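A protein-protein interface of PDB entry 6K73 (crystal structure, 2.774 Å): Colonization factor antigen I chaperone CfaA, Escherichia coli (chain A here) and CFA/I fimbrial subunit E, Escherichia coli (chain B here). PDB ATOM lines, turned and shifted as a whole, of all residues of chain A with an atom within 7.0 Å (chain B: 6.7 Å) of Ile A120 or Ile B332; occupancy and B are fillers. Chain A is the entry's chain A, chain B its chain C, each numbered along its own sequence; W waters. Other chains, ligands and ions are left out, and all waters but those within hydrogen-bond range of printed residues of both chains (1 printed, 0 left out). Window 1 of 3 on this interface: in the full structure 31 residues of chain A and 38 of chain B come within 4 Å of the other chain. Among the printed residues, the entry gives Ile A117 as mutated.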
ATOM      1  N   ALA A   1      -7.455   2.419  34.036  1.00  0.00           N
ATOM      2  CA  ALA A   1      -6.801   2.370  32.733  1.00  0.00           C
ATOM      3  C   ALA A   1      -5.894   1.149  32.615  1.00  0.00           C
ATOM      4  O   ALA A   1      -5.056   0.901  33.481  1.00  0.00           O
ATOM      5  CB  ALA A   1      -6.011   3.647  32.489  1.00  0.00           C
ATOM      6  N   PHE A   3      -4.919   0.222  29.136  1.00  0.00           N
ATOM      7  CA  PHE A   3      -4.415   0.315  27.794  1.00  0.00           C
ATOM      8  C   PHE A   3      -3.917   1.635  27.405  1.00  0.00           C
ATOM      9  O   PHE A   3      -3.918   2.568  28.139  1.00  0.00           O
ATOM     10  CB  PHE A   3      -5.519  -0.006  26.828  1.00  0.00           C
ATOM     11  CG  PHE A   3      -6.613   0.978  26.831  1.00  0.00           C
ATOM     12  CD1 PHE A   3      -7.565   0.942  27.762  1.00  0.00           C
ATOM     13  CD2 PHE A   3      -6.663   1.933  25.893  1.00  0.00           C
ATOM     14  CE1 PHE A   3      -8.557   1.857  27.757  1.00  0.00           C
ATOM     15  CE2 PHE A   3      -7.648   2.847  25.877  1.00  0.00           C
ATOM     16  CZ  PHE A   3      -8.605   2.807  26.802  1.00  0.00           C
ATOM     17  N   LYS A  33     -14.436   0.018  23.275  1.00  0.00           N
ATOM     18  CA  LYS A  33     -15.396   0.591  22.344  1.00  0.00           C
ATOM     19  C   LYS A  33     -14.782   1.831  21.712  1.00  0.00           C
ATOM     20  O   LYS A  33     -14.052   2.580  22.368  1.00  0.00           O
ATOM     21  CB  LYS A  33     -16.724   0.940  23.037  1.00  0.00           C
ATOM     22  CG  LYS A  33     -16.678   2.159  23.951  1.00  0.00           C
ATOM     23  CD  LYS A  33     -17.966   2.320  24.756  1.00  0.00           C
ATOM     24  CE  LYS A  33     -19.152   2.725  23.888  1.00  0.00           C
ATOM     25  NZ  LYS A  33     -20.320   3.120  24.731  1.00  0.00           N
ATOM     26  N   TYR A  35     -15.582   5.267  19.221  1.00  0.00           N
ATOM     27  CA  TYR A  35     -16.614   6.153  18.709  1.00  0.00           C
ATOM     28  C   TYR A  35     -15.994   7.490  18.350  1.00  0.00           C
ATOM     29  O   TYR A  35     -14.950   7.881  18.880  1.00  0.00           O
ATOM     30  CB  TYR A  35     -17.773   6.323  19.705  1.00  0.00           C
ATOM     31  CG  TYR A  35     -17.384   6.778  21.097  1.00  0.00           C
ATOM     32  CD1 TYR A  35     -16.790   5.904  21.998  1.00  0.00           C
ATOM     33  CD2 TYR A  35     -17.651   8.074  21.525  1.00  0.00           C
ATOM     34  CE1 TYR A  35     -16.447   6.314  23.278  1.00  0.00           C
ATOM     35  CE2 TYR A  35     -17.314   8.491  22.803  1.00  0.00           C
ATOM     36  CZ  TYR A  35     -16.714   7.608  23.674  1.00  0.00           C
ATOM     37  OH  TYR A  35     -16.376   8.021  24.942  1.00  0.00           O
ATOM     38  N   VAL A  92     -11.626  10.590  17.953  1.00  0.00           N
ATOM     39  CA  VAL A  92     -12.004   9.186  18.012  1.00  0.00           C
ATOM     40  C   VAL A  92     -11.663   8.691  19.412  1.00  0.00           C
ATOM     41  O   VAL A  92     -10.486   8.580  19.773  1.00  0.00           O
ATOM     42  CB  VAL A  92     -11.295   8.360  16.931  1.00  0.00           C
ATOM     43  CG1 VAL A  92     -11.914   6.987  16.824  1.00  0.00           C
ATOM     44  CG2 VAL A  92     -11.369   9.076  15.589  1.00  0.00           C
ATOM     45  N   TYR A  93     -12.691   8.399  20.200  1.00  0.00           N
ATOM     46  CA  TYR A  93     -12.527   8.011  21.591  1.00  0.00           C
ATOM     47  C   TYR A  93     -12.413   6.500  21.715  1.00  0.00           C
ATOM     48  O   TYR A  93     -13.042   5.746  20.966  1.00  0.00           O
ATOM     49  CB  TYR A  93     -13.699   8.520  22.435  1.00  0.00           C
ATOM     50  CG  TYR A  93     -13.846  10.025  22.430  1.00  0.00           C
ATOM     51  CD1 TYR A  93     -14.356  10.689  21.322  1.00  0.00           C
ATOM     52  CD2 TYR A  93     -13.485  10.784  23.535  1.00  0.00           C
ATOM     53  CE1 TYR A  93     -14.490  12.058  21.308  1.00  0.00           C
ATOM     54  CE2 TYR A  93     -13.620  12.161  23.532  1.00  0.00           C
ATOM     55  CZ  TYR A  93     -14.122  12.789  22.416  1.00  0.00           C
ATOM     56  OH  TYR A  93     -14.256  14.156  22.413  1.00  0.00           O
ATOM     57  N   PHE A  94     -11.614   6.095  22.675  1.00  0.00           N
ATOM     58  CA  PHE A  94     -11.365   4.721  22.991  1.00  0.00           C
ATOM     59  C   PHE A  94     -11.667   4.445  24.433  1.00  0.00           C
ATOM     60  O   PHE A  94     -10.822   4.483  25.268  1.00  0.00           O
ATOM     61  CB  PHE A  94      -9.930   4.378  22.721  1.00  0.00           C
ATOM     62  CG  PHE A  94      -9.571   4.424  21.292  1.00  0.00           C
ATOM     63  CD1 PHE A  94      -9.244   5.586  20.709  1.00  0.00           C
ATOM     64  CD2 PHE A  94      -9.543   3.307  20.555  1.00  0.00           C
ATOM     65  CE1 PHE A  94      -8.929   5.655  19.410  1.00  0.00           C
ATOM     66  CE2 PHE A  94      -9.217   3.363  19.246  1.00  0.00           C
ATOM     67  CZ  PHE A  94      -8.900   4.537  18.675  1.00  0.00           C
ATOM     68  N   GLU A  95     -12.908   4.151  24.713  1.00  0.00           N
ATOM     69  CA  GLU A  95     -13.316   3.870  26.052  1.00  0.00           C
ATOM     70  C   GLU A  95     -13.324   2.385  26.254  1.00  0.00           C
ATOM     71  O   GLU A  95     -13.249   1.652  25.322  1.00  0.00           O
ATOM     72  CB  GLU A  95     -14.711   4.407  26.260  1.00  0.00           C
ATOM     73  CG  GLU A  95     -15.214   4.290  27.659  1.00  0.00           C
ATOM     74  CD  GLU A  95     -16.492   5.019  27.879  1.00  0.00           C
ATOM     75  OE1 GLU A  95     -17.045   5.575  26.954  1.00  0.00           O
ATOM     76  OE2 GLU A  95     -16.961   5.032  29.004  1.00  0.00           O
ATOM     77  N   ALA A  96     -13.425   1.949  27.484  1.00  0.00           N
ATOM     78  CA  ALA A  96     -13.441   0.568  27.751  1.00  0.00           C
ATOM     79  C   ALA A  96     -14.734   0.221  28.375  1.00  0.00           C
ATOM     80  O   ALA A  96     -15.394   1.030  28.882  1.00  0.00           O
ATOM     81  CB  ALA A  96     -12.321   0.245  28.661  1.00  0.00           C
ATOM     82  N   ILE A 117     -11.932   4.980  38.976  1.00  0.00           N
ATOM     83  CA  ILE A 117     -11.263   5.978  38.149  1.00  0.00           C
ATOM     84  C   ILE A 117     -10.951   5.363  36.796  1.00  0.00           C
ATOM     85  O   ILE A 117     -10.454   4.232  36.717  1.00  0.00           O
ATOM     86  CB  ILE A 117      -9.986   6.492  38.839  1.00  0.00           C
ATOM     87  CG1 ILE A 117     -10.354   7.439  39.980  1.00  0.00           C
ATOM     88  CG2 ILE A 117      -9.059   7.159  37.835  1.00  0.00           C
ATOM     89  CD1 ILE A 117     -11.146   8.641  39.537  1.00  0.00           C
ATOM     90  N   ASN A 118     -11.224   6.118  35.730  1.00  0.00           N
ATOM     91  CA  ASN A 118     -11.180   5.572  34.384  1.00  0.00           C
ATOM     92  C   ASN A 118     -10.566   6.546  33.394  1.00  0.00           C
ATOM     93  O   ASN A 118     -10.898   7.736  33.388  1.00  0.00           O
ATOM     94  CB  ASN A 118     -12.572   5.213  33.886  1.00  0.00           C
ATOM     95  CG  ASN A 118     -12.759   3.740  33.775  1.00  0.00           C
ATOM     96  OD1 ASN A 118     -13.095   3.237  32.709  1.00  0.00           O
ATOM     97  ND2 ASN A 118     -12.505   3.024  34.865  1.00  0.00           N
ATOM     98  N   ILE A 119      -9.719   6.009  32.522  1.00  0.00           N
ATOM     99  CA  ILE A 119      -8.957   6.783  31.554  1.00  0.00           C
ATOM    100  C   ILE A 119      -9.506   6.510  30.161  1.00  0.00           C
ATOM    101  O   ILE A 119      -9.726   5.351  29.787  1.00  0.00           O
ATOM    102  CB  ILE A 119      -7.461   6.440  31.633  1.00  0.00           C
ATOM    103  CG1 ILE A 119      -6.884   6.908  32.970  1.00  0.00           C
ATOM    104  CG2 ILE A 119      -6.714   7.047  30.461  1.00  0.00           C
ATOM    105  CD1 ILE A 119      -6.975   8.398  33.174  1.00  0.00           C
ATOM    106  N   ILE A 120      -9.722   7.577  29.393  1.00  0.00           N
ATOM    107  CA  ILE A 120     -10.195   7.492  28.016  1.00  0.00           C
ATOM    108  C   ILE A 120      -9.240   8.278  27.131  1.00  0.00           C
ATOM    109  O   ILE A 120      -8.810   9.380  27.490  1.00  0.00           O
ATOM    110  CB  ILE A 120     -11.632   8.037  27.873  1.00  0.00           C
ATOM    111  CG1 ILE A 120     -12.582   7.314  28.826  1.00  0.00           C
ATOM    112  CG2 ILE A 120     -12.124   7.903  26.441  1.00  0.00           C
ATOM    113  CD1 ILE A 120     -14.015   7.801  28.728  1.00  0.00           C
ATOM    114  N   TYR A 121      -8.915   7.713  25.973  1.00  0.00           N
ATOM    115  CA  TYR A 121      -8.096   8.381  24.971  1.00  0.00           C
ATOM    116  C   TYR A 121      -8.964   8.822  23.805  1.00  0.00           C
ATOM    117  O   TYR A 121      -9.888   8.109  23.398  1.00  0.00           O
ATOM    118  CB  TYR A 121      -6.973   7.471  24.467  1.00  0.00           C
ATOM    119  CG  TYR A 121      -5.911   7.220  25.504  1.00  0.00           C
ATOM    120  CD1 TYR A 121      -4.976   8.197  25.812  1.00  0.00           C
ATOM    121  CD2 TYR A 121      -5.849   6.016  26.185  1.00  0.00           C
ATOM    122  CE1 TYR A 121      -4.007   7.975  26.769  1.00  0.00           C
ATOM    123  CE2 TYR A 121      -4.882   5.786  27.143  1.00  0.00           C
ATOM    124  CZ  TYR A 121      -3.964   6.769  27.430  1.00  0.00           C
ATOM    125  OH  TYR A 121      -3.000   6.540  28.385  1.00  0.00           O
ATOM    126  N   ALA A 122      -8.666  10.007  23.284  1.00  0.00           N
ATOM    127  CA  ALA A 122      -9.316  10.527  22.090  1.00  0.00           C
ATOM    128  C   ALA A 122      -8.226  11.001  21.146  1.00  0.00           C
ATOM    129  O   ALA A 122      -7.460  11.910  21.480  1.00  0.00           O
ATOM    130  CB  ALA A 122     -10.279  11.668  22.432  1.00  0.00           C
ATOM    131  N   ILE B 187      -0.557   7.264  30.048  1.00  0.00           N
ATOM    132  CA  ILE B 187      -0.915   7.535  31.437  1.00  0.00           C
ATOM    133  C   ILE B 187      -1.066   6.229  32.203  1.00  0.00           C
ATOM    134  O   ILE B 187      -1.513   5.304  31.637  1.00  0.00           O
ATOM    135  CB  ILE B 187      -2.273   8.200  31.475  1.00  0.00           C
ATOM    136  CG1 ILE B 187      -2.186   9.534  30.825  1.00  0.00           C
ATOM    137  CG2 ILE B 187      -2.719   8.446  32.873  1.00  0.00           C
ATOM    138  CD1 ILE B 187      -1.193  10.423  31.497  1.00  0.00           C
ATOM    139  N   LEU B 189      -1.866   3.955  36.261  1.00  0.00           N
ATOM    140  CA  LEU B 189      -2.027   4.402  37.633  1.00  0.00           C
ATOM    141  C   LEU B 189      -1.316   3.240  37.998  1.00  0.00           C
ATOM    142  O   LEU B 189      -1.834   2.198  37.836  1.00  0.00           O
ATOM    143  CB  LEU B 189      -3.474   4.488  37.975  1.00  0.00           C
ATOM    144  CG  LEU B 189      -4.063   5.559  37.065  1.00  0.00           C
ATOM    145  CD1 LEU B 189      -5.481   5.251  36.790  1.00  0.00           C
ATOM    146  CD2 LEU B 189      -3.889   7.011  37.418  1.00  0.00           C
ATOM    147  N   MET B 218       0.381   8.404  39.672  1.00  0.00           N
ATOM    148  CA  MET B 218       0.208   8.066  38.269  1.00  0.00           C
ATOM    149  C   MET B 218       1.490   8.290  37.477  1.00  0.00           C
ATOM    150  O   MET B 218       2.366   9.076  37.848  1.00  0.00           O
ATOM    151  CB  MET B 218      -0.949   8.844  37.633  1.00  0.00           C
ATOM    152  CG  MET B 218      -0.892  10.340  37.813  1.00  0.00           C
ATOM    153  SD  MET B 218      -2.344  11.125  37.101  1.00  0.00           S
ATOM    154  CE  MET B 218      -2.166  10.644  35.387  1.00  0.00           C
ATOM    155  N   ILE B 233      -7.073  17.653  28.916  1.00  0.00           N
ATOM    156  CA  ILE B 233      -7.558  16.665  29.869  1.00  0.00           C
ATOM    157  C   ILE B 233      -8.913  17.124  30.386  1.00  0.00           C
ATOM    158  O   ILE B 233      -9.110  18.311  30.669  1.00  0.00           O
ATOM    159  CB  ILE B 233      -6.575  16.462  31.038  1.00  0.00           C
ATOM    160  CG1 ILE B 233      -5.170  16.181  30.507  1.00  0.00           C
ATOM    161  CG2 ILE B 233      -7.037  15.329  31.939  1.00  0.00           C
ATOM    162  CD1 ILE B 233      -4.112  16.162  31.580  1.00  0.00           C
ATOM    163  N   ARG B 234      -9.844  16.180  30.518  1.00  0.00           N
ATOM    164  CA  ARG B 234     -11.190  16.466  30.992  1.00  0.00           C
ATOM    165  C   ARG B 234     -11.547  15.522  32.127  1.00  0.00           C
ATOM    166  O   ARG B 234     -11.178  14.344  32.110  1.00  0.00           O
ATOM    167  CB  ARG B 234     -12.229  16.335  29.867  1.00  0.00           C
ATOM    168  CG  ARG B 234     -12.022  17.304  28.718  1.00  0.00           C
ATOM    169  CD  ARG B 234     -11.136  16.705  27.640  1.00  0.00           C
ATOM    170  NE  ARG B 234     -11.918  16.048  26.599  1.00  0.00           N
ATOM    171  CZ  ARG B 234     -12.140  16.569  25.398  1.00  0.00           C
ATOM    172  NH1 ARG B 234     -11.625  17.749  25.082  1.00  0.00           N
ATOM    173  NH2 ARG B 234     -12.868  15.908  24.508  1.00  0.00           N
ATOM    174  N   PHE B 235     -12.246  16.035  33.113  1.00  0.00           N
ATOM    175  CA  PHE B 235     -12.638  15.227  34.222  1.00  0.00           C
ATOM    176  C   PHE B 235     -14.101  15.262  34.264  1.00  0.00           C
ATOM    177  O   PHE B 235     -14.646  16.304  34.215  1.00  0.00           O
ATOM    178  CB  PHE B 235     -12.114  15.819  35.480  1.00  0.00           C
ATOM    179  CG  PHE B 235     -10.668  15.784  35.561  1.00  0.00           C
ATOM    180  CD1 PHE B 235      -9.945  16.770  35.036  1.00  0.00           C
ATOM    181  CD2 PHE B 235     -10.050  14.742  36.128  1.00  0.00           C
ATOM    182  CE1 PHE B 235      -8.612  16.733  35.084  1.00  0.00           C
ATOM    183  CE2 PHE B 235      -8.713  14.695  36.207  1.00  0.00           C
ATOM    184  CZ  PHE B 235      -7.990  15.697  35.675  1.00  0.00           C
ATOM    185  N   GLN B 236     -14.729  14.117  34.334  1.00  0.00           N
ATOM    186  CA  GLN B 236     -16.151  14.091  34.384  1.00  0.00           C
ATOM    187  C   GLN B 236     -16.763  12.979  35.177  1.00  0.00           C
ATOM    188  O   GLN B 236     -16.269  11.906  35.255  1.00  0.00           O
ATOM    189  CB  GLN B 236     -16.708  14.185  32.977  1.00  0.00           C
ATOM    190  CG  GLN B 236     -17.387  12.964  32.400  1.00  0.00           C
ATOM    191  CD  GLN B 236     -17.890  13.218  31.017  1.00  0.00           C
ATOM    192  OE1 GLN B 236     -17.119  13.391  30.084  1.00  0.00           O
ATOM    193  NE2 GLN B 236     -19.193  13.256  30.874  1.00  0.00           N
ATOM    194  N   LEU B 262     -11.609  17.046  43.463  1.00  0.00           N
ATOM    195  CA  LEU B 262     -10.357  16.475  42.987  1.00  0.00           C
ATOM    196  C   LEU B 262      -9.315  17.571  42.813  1.00  0.00           C
ATOM    197  O   LEU B 262      -9.643  18.726  42.518  1.00  0.00           O
ATOM    198  CB  LEU B 262     -10.515  15.733  41.646  1.00  0.00           C
ATOM    199  CG  LEU B 262     -11.894  15.417  41.073  1.00  0.00           C
ATOM    200  CD1 LEU B 262     -11.744  14.957  39.633  1.00  0.00           C
ATOM    201  CD2 LEU B 262     -12.596  14.356  41.894  1.00  0.00           C
ATOM    202  N   LEU B 312      -3.323  12.474  41.393  1.00  0.00           N
ATOM    203  CA  LEU B 312      -4.692  12.916  41.600  1.00  0.00           C
ATOM    204  C   LEU B 312      -5.070  12.647  43.049  1.00  0.00           C
ATOM    205  O   LEU B 312      -4.832  11.552  43.567  1.00  0.00           O
ATOM    206  CB  LEU B 312      -5.665  12.197  40.668  1.00  0.00           C
ATOM    207  CG  LEU B 312      -7.085  12.761  40.779  1.00  0.00           C
ATOM    208  CD1 LEU B 312      -7.175  14.114  40.082  1.00  0.00           C
ATOM    209  CD2 LEU B 312      -8.124  11.793  40.240  1.00  0.00           C
ATOM    210  N   ILE B 330     -15.511   8.195  37.587  1.00  0.00           N
ATOM    211  CA  ILE B 330     -14.942   9.401  36.998  1.00  0.00           C
ATOM    212  C   ILE B 330     -14.190   9.030  35.729  1.00  0.00           C
ATOM    213  O   ILE B 330     -13.301   8.172  35.753  1.00  0.00           O
ATOM    214  CB  ILE B 330     -14.018  10.139  37.989  1.00  0.00           C
ATOM    215  CG1 ILE B 330     -14.859  10.898  39.020  1.00  0.00           C
ATOM    216  CG2 ILE B 330     -13.055  11.065  37.256  1.00  0.00           C
ATOM    217  CD1 ILE B 330     -14.221  12.173  39.532  1.00  0.00           C
ATOM    218  N   LYS B 331     -14.552   9.677  34.625  1.00  0.00           N
ATOM    219  CA  LYS B 331     -13.871   9.522  33.347  1.00  0.00           C
ATOM    220  C   LYS B 331     -12.852  10.643  33.188  1.00  0.00           C
ATOM    221  O   LYS B 331     -13.173  11.813  33.407  1.00  0.00           O
ATOM    222  CB  LYS B 331     -14.875   9.542  32.195  1.00  0.00           C
ATOM    223  CG  LYS B 331     -15.950   8.475  32.295  1.00  0.00           C
ATOM    224  CD  LYS B 331     -15.345   7.086  32.229  1.00  0.00           C
ATOM    225  CE  LYS B 331     -16.420   6.024  32.300  1.00  0.00           C
ATOM    226  NZ  LYS B 331     -17.431   6.229  31.231  1.00  0.00           N
ATOM    227  N   ILE B 332     -11.629  10.278  32.811  1.00  0.00           N
ATOM    228  CA  ILE B 332     -10.534  11.223  32.611  1.00  0.00           C
ATOM    229  C   ILE B 332     -10.056  11.051  31.174  1.00  0.00           C
ATOM    230  O   ILE B 332      -9.379  10.068  30.850  1.00  0.00           O
ATOM    231  CB  ILE B 332      -9.394  11.005  33.618  1.00  0.00           C
ATOM    232  CG1 ILE B 332      -9.937  11.086  35.047  1.00  0.00           C
ATOM    233  CG2 ILE B 332      -8.281  12.031  33.411  1.00  0.00           C
ATOM    234  CD1 ILE B 332      -9.080  10.379  36.078  1.00  0.00           C
ATOM    235  N   THR B 333     -10.412  12.006  30.316  1.00  0.00           N
ATOM    236  CA  THR B 333     -10.180  11.917  28.877  1.00  0.00           C
ATOM    237  C   THR B 333      -8.881  12.629  28.516  1.00  0.00           C
ATOM    238  O   THR B 333      -8.623  13.738  28.989  1.00  0.00           O
ATOM    239  CB  THR B 333     -11.357  12.526  28.108  1.00  0.00           C
ATOM    240  OG1 THR B 333     -12.424  12.815  29.020  1.00  0.00           O
ATOM    241  CG2 THR B 333     -11.869  11.560  27.044  1.00  0.00           C
ATOM    242  N   PHE B 334      -8.072  11.983  27.676  1.00  0.00           N
ATOM    243  CA  PHE B 334      -6.777  12.500  27.258  1.00  0.00           C
ATOM    244  C   PHE B 334      -6.808  12.773  25.762  1.00  0.00           C
ATOM    245  O   PHE B 334      -7.129  11.879  24.972  1.00  0.00           O
ATOM    246  CB  PHE B 334      -5.655  11.530  27.617  1.00  0.00           C
ATOM    247  CG  PHE B 334      -5.154  11.712  29.010  1.00  0.00           C
ATOM    248  CD1 PHE B 334      -5.791  11.101  30.075  1.00  0.00           C
ATOM    249  CD2 PHE B 334      -4.072  12.533  29.263  1.00  0.00           C
ATOM    250  CE1 PHE B 334      -5.342  11.287  31.366  1.00  0.00           C
ATOM    251  CE2 PHE B 334      -3.621  12.728  30.547  1.00  0.00           C
ATOM    252  CZ  PHE B 334      -4.256  12.103  31.604  1.00  0.00           C
ATOM    253  N   THR B 335      -6.479  14.006  25.382  1.00  0.00           N
ATOM    254  CA  THR B 335      -6.641  14.456  24.011  1.00  0.00           C
ATOM    255  C   THR B 335      -5.646  15.564  23.731  1.00  0.00           C
ATOM    256  O   THR B 335      -5.360  16.376  24.621  1.00  0.00           O
ATOM    257  CB  THR B 335      -8.061  14.987  23.751  1.00  0.00           C
ATOM    258  OG1 THR B 335      -8.984  14.392  24.670  1.00  0.00           O
ATOM    259  CG2 THR B 335      -8.486  14.661  22.347  1.00  0.00           C
HETATM  260  O   HOH W   1      -3.680   4.526  29.537  1.00  0.00           O
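OH of Tyr A93 sits at hydrogen-bond distance from NH2 of Arg B234 (3.1 Å). The side-chain amino group (NZ) of Lys B331 is in salt-bridge range of the side-chain carboxylate (OE2) of Glu A95. The backbone NH (N) of Asn A118 sits at hydrogen-bond distance from the backbone carbonyl oxygen (O) of Ile B330, 2.9 Å away. The backbone carbonyl oxygen of Asn A118 is in hydrogen-bond range of the backbone NH of Ile B332, 2.7 Å away. The backbone NH (N) of Ile A120 is in hydrogen-bond range of the backbone carbonyl oxygen (O) of Ile B332 (2.9 Å). The backbone carbonyl oxygen (O) of Ile A120 sits at hydrogen-bond distance from the backbone NH (N) of Phe B334, at 2.7 Å. N of Ile B187 lies within hydrogen-bond range of OH of Tyr A121 (3.0 Å). N of Ala A122 sits at hydrogen-bond distance from O of Phe B334, at 3.0 Å.
O of Glu A95 lies within hydrogen-bond range of N of Lys A33 (2.9 Å). O of Tyr A35 lies within hydrogen-bond range of N of Tyr A93 (2.7 Å). The side-chain hydroxyl of Tyr A35 lies within hydrogen-bond range of the side-chain carboxylate of Glu A95. N of Phe A94 sits at hydrogen-bond distance from O of Tyr A121. The backbone carbonyl oxygen (O) of Arg B234 is in hydrogen-bond range of the backbone NH (N) of Thr B333 (3.0 Å). O of Gln B236 is in hydrogen-bond range of N of Lys B331 (2.9 Å).
Among the printed residues, pairs that only touch across the chains: Ala A122 with Thr B335 (3.1 Å), Ile A120 with Thr B333 (3.2 Å), Ile A119 with Ile B332 (3.4 Å), Asn A118 with Lys B331 (3.5 Å), Ile A117 with Ile B330 (3.6 Å), Tyr A121 with Phe B334 (3.6 Å), Ile A117 with Ile B332 (3.7 Å), Ile A119 with Phe B334 (3.8 Å), Ile A120 with Lys B331 (3.8 Å) and Tyr A93 with Thr B333 (3.9 Å).
Of chain B, only Lys B331, Ile B332, Thr B333 and Phe B334 come within 4 Å of Ile A120. Of chain A, only Ile A117 (3.7 Å), Asn A118 (2.7 Å), Ile A119 (3.4 Å) and Ile A120 (2.9 Å) come within 4 Å of Ile B332. Of the printed residues of chain A, Arg B234 touches Tyr A93. Of the printed residues of chain A, Phe B334 touches Ile A119, Ile A120, Tyr A121 and Ala A122. Of the printed residues of chain A, Lys B331 touches Glu A95 (2.6 Å), Asn A118 (3.5 Å) and Ile A120 (3.8 Å). The nearest residue of chain B that does not touch Ile A120 is Thr B335 (5.6 Å). The nearest residue of chain A that does not touch Ile B332 is Tyr A121 (5.4 Å). The nearest printed residue of chain B that does not touch Glu A95 is Thr B333 (7.7 Å).
Of the 15 printed residues of chain A, 8 touch a printed residue of chain B. Hydrophobic or aromatic side chains of chain A within 4 Å of the printed part of chain B: Tyr A93, Ile A117, Ile A119, Ile A120, Tyr A121 and Ala A122. Of the 15 printed residues of chain B, 8 touch a printed residue of chain A. Along chain B the printed residues that touch a printed residue of chain A span positions 187 to 335. Among the printed residues, Asp or Glu carboxylates within 4 Å of a Lys or Arg side-chain nitrogen of the other chain: Glu A95 with Lys B331.
Water W1 lies within hydrogen-bond range of OH of Tyr A121 (2.4 Å), O of Phe A3 (2.4 Å) and O of Ile B187 (3.1 Å).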
